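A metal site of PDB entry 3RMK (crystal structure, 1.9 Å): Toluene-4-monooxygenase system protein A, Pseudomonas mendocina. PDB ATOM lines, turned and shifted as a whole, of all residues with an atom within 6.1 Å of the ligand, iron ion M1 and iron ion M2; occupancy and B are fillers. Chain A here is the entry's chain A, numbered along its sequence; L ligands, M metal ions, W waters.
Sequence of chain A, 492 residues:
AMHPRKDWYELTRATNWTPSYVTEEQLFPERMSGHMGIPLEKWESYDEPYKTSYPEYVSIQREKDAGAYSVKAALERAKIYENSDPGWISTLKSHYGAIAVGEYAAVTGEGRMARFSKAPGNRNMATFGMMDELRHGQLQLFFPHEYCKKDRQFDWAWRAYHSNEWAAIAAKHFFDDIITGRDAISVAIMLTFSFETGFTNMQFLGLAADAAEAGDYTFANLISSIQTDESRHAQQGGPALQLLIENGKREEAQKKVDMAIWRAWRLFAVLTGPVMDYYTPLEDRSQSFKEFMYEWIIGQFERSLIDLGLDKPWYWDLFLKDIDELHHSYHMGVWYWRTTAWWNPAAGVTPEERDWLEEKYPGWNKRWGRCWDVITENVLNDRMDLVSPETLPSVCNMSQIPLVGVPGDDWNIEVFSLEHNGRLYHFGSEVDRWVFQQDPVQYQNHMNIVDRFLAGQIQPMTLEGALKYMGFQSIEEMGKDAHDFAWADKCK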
ATOM      1  N   ALA A  98     -27.900 -21.698  34.873  1.00  0.00           N
ATOM      2  CA  ALA A  98     -27.925 -22.672  33.788  1.00  0.00           C
ATOM      3  C   ALA A  98     -26.595 -23.374  33.561  1.00  0.00           C
ATOM      4  O   ALA A  98     -26.561 -24.494  33.056  1.00  0.00           O
ATOM      5  CB  ALA A  98     -28.346 -21.991  32.493  1.00  0.00           C
ATOM      6  N   ILE A  99     -25.508 -22.705  33.937  1.00  0.00           N
ATOM      7  CA  ILE A  99     -24.176 -23.156  33.528  1.00  0.00           C
ATOM      8  C   ILE A  99     -23.274 -23.743  34.619  1.00  0.00           C
ATOM      9  O   ILE A  99     -22.536 -24.699  34.356  1.00  0.00           O
ATOM     10  CB  ILE A  99     -23.400 -22.017  32.827  1.00  0.00           C
ATOM     11  CG1 ILE A  99     -24.113 -21.606  31.528  1.00  0.00           C
ATOM     12  CG2 ILE A  99     -21.962 -22.453  32.533  1.00  0.00           C
ATOM     13  CD1 ILE A  99     -24.296 -22.772  30.543  1.00  0.00           C
ATOM     14  N   GLY A 102     -23.644 -27.385  35.612  1.00  0.00           N
ATOM     15  CA  GLY A 102     -23.455 -28.086  34.343  1.00  0.00           C
ATOM     16  C   GLY A 102     -21.990 -28.188  33.947  1.00  0.00           C
ATOM     17  O   GLY A 102     -21.564 -29.216  33.416  1.00  0.00           O
ATOM     18  N   GLU A 103     -21.207 -27.120  34.174  1.00  0.00           N
ATOM     19  CA  GLU A 103     -19.757 -27.214  33.957  1.00  0.00           C
ATOM     20  C   GLU A 103     -19.218 -28.357  34.810  1.00  0.00           C
ATOM     21  O   GLU A 103     -18.426 -29.160  34.331  1.00  0.00           O
ATOM     22  CB  GLU A 103     -19.021 -25.932  34.332  1.00  0.00           C
ATOM     23  CG  GLU A 103     -19.387 -24.703  33.492  1.00  0.00           C
ATOM     24  CD  GLU A 103     -18.392 -24.416  32.382  1.00  0.00           C
ATOM     25  OE1 GLU A 103     -17.585 -25.318  32.046  1.00  0.00           O
ATOM     26  OE2 GLU A 103     -18.418 -23.278  31.868  1.00  0.00           O
ATOM     27  N   ALA A 106     -19.907 -31.636  33.387  1.00  0.00           N
ATOM     28  CA  ALA A 106     -19.034 -31.949  32.252  1.00  0.00           C
ATOM     29  C   ALA A 106     -17.733 -32.647  32.690  1.00  0.00           C
ATOM     30  O   ALA A 106     -17.095 -33.333  31.889  1.00  0.00           O
ATOM     31  CB  ALA A 106     -18.722 -30.695  31.421  1.00  0.00           C
ATOM     32  N   GLU A 110     -16.105 -35.856  30.607  1.00  0.00           N
ATOM     33  CA  GLU A 110     -14.662 -35.984  30.384  1.00  0.00           C
ATOM     34  C   GLU A 110     -14.100 -37.256  31.033  1.00  0.00           C
ATOM     35  O   GLU A 110     -13.339 -37.976  30.411  1.00  0.00           O
ATOM     36  CB  GLU A 110     -13.943 -34.729  30.864  1.00  0.00           C
ATOM     37  CG  GLU A 110     -14.365 -33.452  30.082  1.00  0.00           C
ATOM     38  CD  GLU A 110     -13.742 -33.379  28.680  1.00  0.00           C
ATOM     39  OE1 GLU A 110     -12.839 -34.169  28.396  1.00  0.00           O
ATOM     40  OE2 GLU A 110     -14.151 -32.520  27.861  1.00  0.00           O
ATOM     41  N   ASP A 132     -10.160 -28.958  33.457  1.00  0.00           N
ATOM     42  CA  ASP A 132     -10.724 -27.724  32.926  1.00  0.00           C
ATOM     43  C   ASP A 132     -12.131 -27.512  33.450  1.00  0.00           C
ATOM     44  O   ASP A 132     -12.483 -26.406  33.874  1.00  0.00           O
ATOM     45  CB  ASP A 132     -10.785 -27.741  31.390  1.00  0.00           C
ATOM     46  CG  ASP A 132      -9.431 -27.556  30.752  1.00  0.00           C
ATOM     47  OD1 ASP A 132      -8.459 -27.173  31.453  1.00  0.00           O
ATOM     48  OD2 ASP A 132      -9.339 -27.790  29.528  1.00  0.00           O
ATOM     49  N   GLU A 133     -12.944 -28.548  33.383  1.00  0.00           N
ATOM     50  CA  GLU A 133     -14.354 -28.371  33.733  1.00  0.00           C
ATOM     51  C   GLU A 133     -14.485 -28.216  35.249  1.00  0.00           C
ATOM     52  O   GLU A 133     -15.380 -27.527  35.734  1.00  0.00           O
ATOM     53  CB  GLU A 133     -15.225 -29.496  33.170  1.00  0.00           C
ATOM     54  CG  GLU A 133     -15.170 -29.644  31.623  1.00  0.00           C
ATOM     55  CD  GLU A 133     -15.576 -28.365  30.848  1.00  0.00           C
ATOM     56  OE1 GLU A 133     -15.731 -27.284  31.452  1.00  0.00           O
ATOM     57  OE2 GLU A 133     -15.717 -28.451  29.617  1.00  0.00           O
ATOM     58  N   HIS A 136     -13.920 -24.641  35.802  1.00  0.00           N
ATOM     59  CA  HIS A 136     -15.024 -23.787  35.361  1.00  0.00           C
ATOM     60  C   HIS A 136     -16.191 -23.889  36.301  1.00  0.00           C
ATOM     61  O   HIS A 136     -16.895 -22.902  36.519  1.00  0.00           O
ATOM     62  CB  HIS A 136     -15.422 -24.103  33.900  1.00  0.00           C
ATOM     63  CG  HIS A 136     -14.292 -23.930  32.936  1.00  0.00           C
ATOM     64  ND1 HIS A 136     -14.306 -24.433  31.656  1.00  0.00           N
ATOM     65  CD2 HIS A 136     -13.075 -23.342  33.097  1.00  0.00           C
ATOM     66  CE1 HIS A 136     -13.170 -24.145  31.053  1.00  0.00           C
ATOM     67  NE2 HIS A 136     -12.402 -23.492  31.909  1.00  0.00           N
ATOM     68  N   GLN A 140     -17.356 -20.631  38.677  1.00  0.00           N
ATOM     69  CA  GLN A 140     -18.722 -20.142  38.482  1.00  0.00           C
ATOM     70  C   GLN A 140     -19.655 -20.467  39.652  1.00  0.00           C
ATOM     71  O   GLN A 140     -20.841 -20.184  39.613  1.00  0.00           O
ATOM     72  CB  GLN A 140     -19.270 -20.604  37.120  1.00  0.00           C
ATOM     73  CG  GLN A 140     -18.617 -19.809  35.987  1.00  0.00           C
ATOM     74  CD  GLN A 140     -18.917 -20.312  34.579  1.00  0.00           C
ATOM     75  OE1 GLN A 140     -19.564 -19.625  33.790  1.00  0.00           O
ATOM     76  NE2 GLN A 140     -18.379 -21.484  34.257  1.00  0.00           N
ATOM     77  N   TYR A 161     -29.732 -26.853  39.430  1.00  0.00           N
ATOM     78  CA  TYR A 161     -29.624 -28.271  39.035  1.00  0.00           C
ATOM     79  C   TYR A 161     -30.153 -29.212  40.128  1.00  0.00           C
ATOM     80  O   TYR A 161     -30.351 -30.408  39.888  1.00  0.00           O
ATOM     81  CB  TYR A 161     -28.185 -28.630  38.672  1.00  0.00           C
ATOM     82  CG  TYR A 161     -27.773 -28.183  37.279  1.00  0.00           C
ATOM     83  CD1 TYR A 161     -27.814 -26.845  36.902  1.00  0.00           C
ATOM     84  CD2 TYR A 161     -27.320 -29.118  36.352  1.00  0.00           C
ATOM     85  CE1 TYR A 161     -27.426 -26.439  35.634  1.00  0.00           C
ATOM     86  CE2 TYR A 161     -26.929 -28.727  35.069  1.00  0.00           C
ATOM     87  CZ  TYR A 161     -26.982 -27.392  34.717  1.00  0.00           C
ATOM     88  OH  TYR A 161     -26.593 -27.027  33.446  1.00  0.00           O
ATOM     89  N   PHE A 175     -28.225 -31.809  29.059  1.00  0.00           N
ATOM     90  CA  PHE A 175     -26.853 -32.154  29.478  1.00  0.00           C
ATOM     91  C   PHE A 175     -26.700 -33.602  29.938  1.00  0.00           C
ATOM     92  O   PHE A 175     -25.650 -34.226  29.747  1.00  0.00           O
ATOM     93  CB  PHE A 175     -26.346 -31.192  30.564  1.00  0.00           C
ATOM     94  CG  PHE A 175     -26.131 -29.800  30.061  1.00  0.00           C
ATOM     95  CD1 PHE A 175     -25.381 -29.573  28.920  1.00  0.00           C
ATOM     96  CD2 PHE A 175     -26.680 -28.721  30.730  1.00  0.00           C
ATOM     97  CE1 PHE A 175     -25.193 -28.293  28.440  1.00  0.00           C
ATOM     98  CE2 PHE A 175     -26.474 -27.422  30.260  1.00  0.00           C
ATOM     99  CZ  PHE A 175     -25.734 -27.217  29.120  1.00  0.00           C
ATOM    100  N   ILE A 179     -23.917 -35.250  27.909  1.00  0.00           N
ATOM    101  CA  ILE A 179     -22.722 -35.236  28.774  1.00  0.00           C
ATOM    102  C   ILE A 179     -22.580 -36.479  29.635  1.00  0.00           C
ATOM    103  O   ILE A 179     -21.578 -37.188  29.539  1.00  0.00           O
ATOM    104  CB  ILE A 179     -22.676 -34.014  29.708  1.00  0.00           C
ATOM    105  CG1 ILE A 179     -22.723 -32.715  28.901  1.00  0.00           C
ATOM    106  CG2 ILE A 179     -21.403 -34.055  30.570  1.00  0.00           C
ATOM    107  CD1 ILE A 179     -22.565 -31.440  29.764  1.00  0.00           C
ATOM    108  N   LEU A 191     -20.886 -33.579  23.056  1.00  0.00           N
ATOM    109  CA  LEU A 191     -20.389 -32.512  23.917  1.00  0.00           C
ATOM    110  C   LEU A 191     -19.269 -31.696  23.267  1.00  0.00           C
ATOM    111  O   LEU A 191     -19.452 -30.536  22.990  1.00  0.00           O
ATOM    112  CB  LEU A 191     -19.943 -33.043  25.284  1.00  0.00           C
ATOM    113  CG  LEU A 191     -19.216 -32.022  26.183  1.00  0.00           C
ATOM    114  CD1 LEU A 191     -20.117 -30.835  26.577  1.00  0.00           C
ATOM    115  CD2 LEU A 191     -18.659 -32.706  27.428  1.00  0.00           C
ATOM    116  N   PHE A 195     -21.556 -29.276  20.991  1.00  0.00           N
ATOM    117  CA  PHE A 195     -21.924 -28.235  21.940  1.00  0.00           C
ATOM    118  C   PHE A 195     -20.820 -27.231  22.250  1.00  0.00           C
ATOM    119  O   PHE A 195     -21.054 -26.016  22.195  1.00  0.00           O
ATOM    120  CB  PHE A 195     -22.454 -28.848  23.244  1.00  0.00           C
ATOM    121  CG  PHE A 195     -22.956 -27.820  24.228  1.00  0.00           C
ATOM    122  CD1 PHE A 195     -24.034 -26.994  23.896  1.00  0.00           C
ATOM    123  CD2 PHE A 195     -22.347 -27.650  25.464  1.00  0.00           C
ATOM    124  CE1 PHE A 195     -24.487 -26.029  24.787  1.00  0.00           C
ATOM    125  CE2 PHE A 195     -22.803 -26.701  26.352  1.00  0.00           C
ATOM    126  CZ  PHE A 195     -23.875 -25.883  26.021  1.00  0.00           C
ATOM    127  N   GLU A 196     -19.632 -27.715  22.593  1.00  0.00           N
ATOM    128  CA  GLU A 196     -18.526 -26.846  22.997  1.00  0.00           C
ATOM    129  C   GLU A 196     -17.898 -26.095  21.834  1.00  0.00           C
ATOM    130  O   GLU A 196     -17.856 -24.871  21.826  1.00  0.00           O
ATOM    131  CB  GLU A 196     -17.457 -27.644  23.768  1.00  0.00           C
ATOM    132  CG  GLU A 196     -17.985 -28.075  25.144  1.00  0.00           C
ATOM    133  CD  GLU A 196     -16.965 -28.861  25.964  1.00  0.00           C
ATOM    134  OE1 GLU A 196     -16.435 -29.859  25.464  1.00  0.00           O
ATOM    135  OE2 GLU A 196     -16.714 -28.485  27.116  1.00  0.00           O
ATOM    136  N   THR A 200     -20.661 -23.115  22.555  1.00  0.00           N
ATOM    137  CA  THR A 200     -20.181 -22.384  23.730  1.00  0.00           C
ATOM    138  C   THR A 200     -18.956 -21.517  23.437  1.00  0.00           C
ATOM    139  O   THR A 200     -18.778 -20.473  24.032  1.00  0.00           O
ATOM    140  CB  THR A 200     -19.890 -23.312  24.931  1.00  0.00           C
ATOM    141  OG1 THR A 200     -18.836 -24.202  24.592  1.00  0.00           O
ATOM    142  CG2 THR A 200     -21.128 -24.133  25.285  1.00  0.00           C
ATOM    143  N   PHE A 204     -19.321 -17.775  24.610  1.00  0.00           N
ATOM    144  CA  PHE A 204     -18.495 -17.179  25.671  1.00  0.00           C
ATOM    145  C   PHE A 204     -17.743 -15.936  25.186  1.00  0.00           C
ATOM    146  O   PHE A 204     -17.657 -14.943  25.891  1.00  0.00           O
ATOM    147  CB  PHE A 204     -17.568 -18.216  26.312  1.00  0.00           C
ATOM    148  CG  PHE A 204     -18.230 -19.040  27.415  1.00  0.00           C
ATOM    149  CD1 PHE A 204     -19.534 -19.477  27.294  1.00  0.00           C
ATOM    150  CD2 PHE A 204     -17.538 -19.358  28.575  1.00  0.00           C
ATOM    151  CE1 PHE A 204     -20.156 -20.234  28.313  1.00  0.00           C
ATOM    152  CE2 PHE A 204     -18.130 -20.115  29.599  1.00  0.00           C
ATOM    153  CZ  PHE A 204     -19.449 -20.542  29.465  1.00  0.00           C
ATOM    154  N   ILE A 226     -12.102 -18.367  31.073  1.00  0.00           N
ATOM    155  CA  ILE A 226     -12.711 -19.665  30.835  1.00  0.00           C
ATOM    156  C   ILE A 226     -12.682 -20.072  29.366  1.00  0.00           C
ATOM    157  O   ILE A 226     -12.374 -21.220  29.028  1.00  0.00           O
ATOM    158  CB  ILE A 226     -14.159 -19.677  31.357  1.00  0.00           C
ATOM    159  CG1 ILE A 226     -14.141 -19.605  32.889  1.00  0.00           C
ATOM    160  CG2 ILE A 226     -14.913 -20.880  30.782  1.00  0.00           C
ATOM    161  CD1 ILE A 226     -15.520 -19.451  33.557  1.00  0.00           C
ATOM    162  N   GLU A 230     -11.133 -23.557  26.406  1.00  0.00           N
ATOM    163  CA  GLU A 230     -12.100 -24.376  25.680  1.00  0.00           C
ATOM    164  C   GLU A 230     -11.475 -25.354  24.690  1.00  0.00           C
ATOM    165  O   GLU A 230     -11.798 -26.537  24.706  1.00  0.00           O
ATOM    166  CB  GLU A 230     -13.180 -23.529  24.979  1.00  0.00           C
ATOM    167  CG  GLU A 230     -14.490 -24.297  24.753  1.00  0.00           C
ATOM    168  CD  GLU A 230     -15.113 -24.772  26.069  1.00  0.00           C
ATOM    169  OE1 GLU A 230     -15.117 -23.989  27.046  1.00  0.00           O
ATOM    170  OE2 GLU A 230     -15.583 -25.934  26.142  1.00  0.00           O
ATOM    171  N   HIS A 233      -9.914 -29.092  25.406  1.00  0.00           N
ATOM    172  CA  HIS A 233     -10.728 -30.313  25.513  1.00  0.00           C
ATOM    173  C   HIS A 233     -11.827 -30.384  24.475  1.00  0.00           C
ATOM    174  O   HIS A 233     -12.306 -31.473  24.135  1.00  0.00           O
ATOM    175  CB  HIS A 233     -11.309 -30.468  26.933  1.00  0.00           C
ATOM    176  CG  HIS A 233     -12.202 -29.338  27.340  1.00  0.00           C
ATOM    177  ND1 HIS A 233     -11.752 -28.273  28.089  1.00  0.00           N
ATOM    178  CD2 HIS A 233     -13.503 -29.087  27.049  1.00  0.00           C
ATOM    179  CE1 HIS A 233     -12.756 -27.423  28.267  1.00  0.00           C
ATOM    180  NE2 HIS A 233     -13.822 -27.893  27.650  1.00  0.00           N
ATOM    181  N   ALA A 234     -12.250 -29.229  23.949  1.00  0.00           N
ATOM    182  CA  ALA A 234     -13.310 -29.226  22.958  1.00  0.00           C
ATOM    183  C   ALA A 234     -12.802 -29.825  21.641  1.00  0.00           C
ATOM    184  O   ALA A 234     -13.597 -30.252  20.810  1.00  0.00           O
ATOM    185  CB  ALA A 234     -13.841 -27.788  22.731  1.00  0.00           C
HETATM  186  O1  LIG L   1     -17.453 -26.305  28.523  1.00  0.00           O
HETATM  187  C1  LIG L   1     -18.714 -26.424  28.998  1.00  0.00           C
HETATM  188  C2  LIG L   1     -19.153 -27.661  29.446  1.00  0.00           C
HETATM  189  C3  LIG L   1     -20.434 -27.792  29.942  1.00  0.00           C
HETATM  190  C4  LIG L   1     -21.269 -26.681  29.987  1.00  0.00           C
HETATM  191  C5  LIG L   1     -20.830 -25.444  29.539  1.00  0.00           C
HETATM  192  C6  LIG L   1     -19.544 -25.324  29.036  1.00  0.00           C
HETATM  193 BR1  LIG L   1     -23.015 -26.871  30.667  1.00  0.00          BR
HETATM  194 FE    FE M   1     -15.733 -27.119  28.071  1.00  0.00          FE
HETATM  195 FE    FE M   2     -16.135 -25.363  30.641  1.00  0.00          FE
HETATM  196  O   HOH W   1     -17.679 -23.719  27.190  1.00  0.00           O
HETATM  197  O   HOH W   2     -16.894 -23.507  29.836  1.00  0.00           O
HETATM  198  O   HOH W   3     -15.111 -25.538  29.075  1.00  0.00           O
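The side-chain hydroxyl of Thr 200 lies within hydrogen-bond range of the backbone carbonyl oxygen of Glu 196 (3.0 Å).
The backbone NH (N) of Glu 196 sits at hydrogen-bond distance from the backbone carbonyl oxygen (O) of Leu 191 (2.9 Å).
OE2 of Glu 103 is in hydrogen-bond range of NE2 of Gln 140 (3.0 Å).
OD2 of Asp 132 is in hydrogen-bond range of ND1 of His 233, at 2.9 Å.
The backbone carbonyl oxygen (O) of Asp 132 sits close to a ring nitrogen (ND1) of His 136 (3.5 Å).
The backbone carbonyl oxygen of His 136 sits at hydrogen-bond distance from the side-chain amide nitrogen of Gln 140, 3.1 Å away.
The backbone NH (N) of Thr 200 is in hydrogen-bond range of the backbone carbonyl oxygen (O) of Phe 195, 2.9 Å away.
C of Gly 102 touches BR1 of the ligand (3.7 Å).
CB of Ala 106 touches C2 of the ligand, at 3.6 Å.
CZ of Phe 175 touches BR1 of the ligand (3.1 Å).
Phe 195 touches the ligand.
Hydrophobic or aromatic side chains that line the ligand: Ala 106, Phe 175 and Phe 195.
Of the 22 residues printed, 8 come within 4 Å of the ligand.
The nearest printed residue that does not touch the ligand is His 233 (4.1 Å).
Of the 22 residues printed, 4 come within 4 Å of iron ion M1.
Of the 22 residues printed, 4 come within 4 Å of iron ion M2.
The nearest printed residue that does not touch iron ion M2 is His 233 (4.5 Å).
Iron ion M1 is bound by the side-chain carboxylate of Glu 196 (1.9 Å), an oxygen (O1) of the ligand (2.0 Å), water W3 (2.0 Å), the side-chain carboxylate of Glu 133 (2.0 Å), a ring nitrogen (NE2) of His 233 (2.1 Å) and the side-chain carboxylate of Glu 230 (2.3 Å).
Iron ion M2 is bound by water W3 (1.9 Å), the side-chain carboxylate (OE1) of Glu 103 (2.0 Å), the side-chain carboxylate (OE1) of Glu 133 (2.1 Å), water W2 (2.2 Å) and a ring nitrogen (ND1) of His 136 (2.3 Å).
Iron ion M2 has five donor atoms within binding distance.
Slightly farther from iron ion M2 lies an oxygen (O1) of the ligand (2.7 Å).
Water W2 bridges the side-chain carboxylate (OE2) of Glu 103 (2.6 Å) and the side-chain carboxylate (OE1) of Glu 230 (3.3 Å).
Water W1 lies within hydrogen-bond range of OE1 of Glu 230 (2.6 Å) and OG1 of Thr 200 (2.9 Å).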
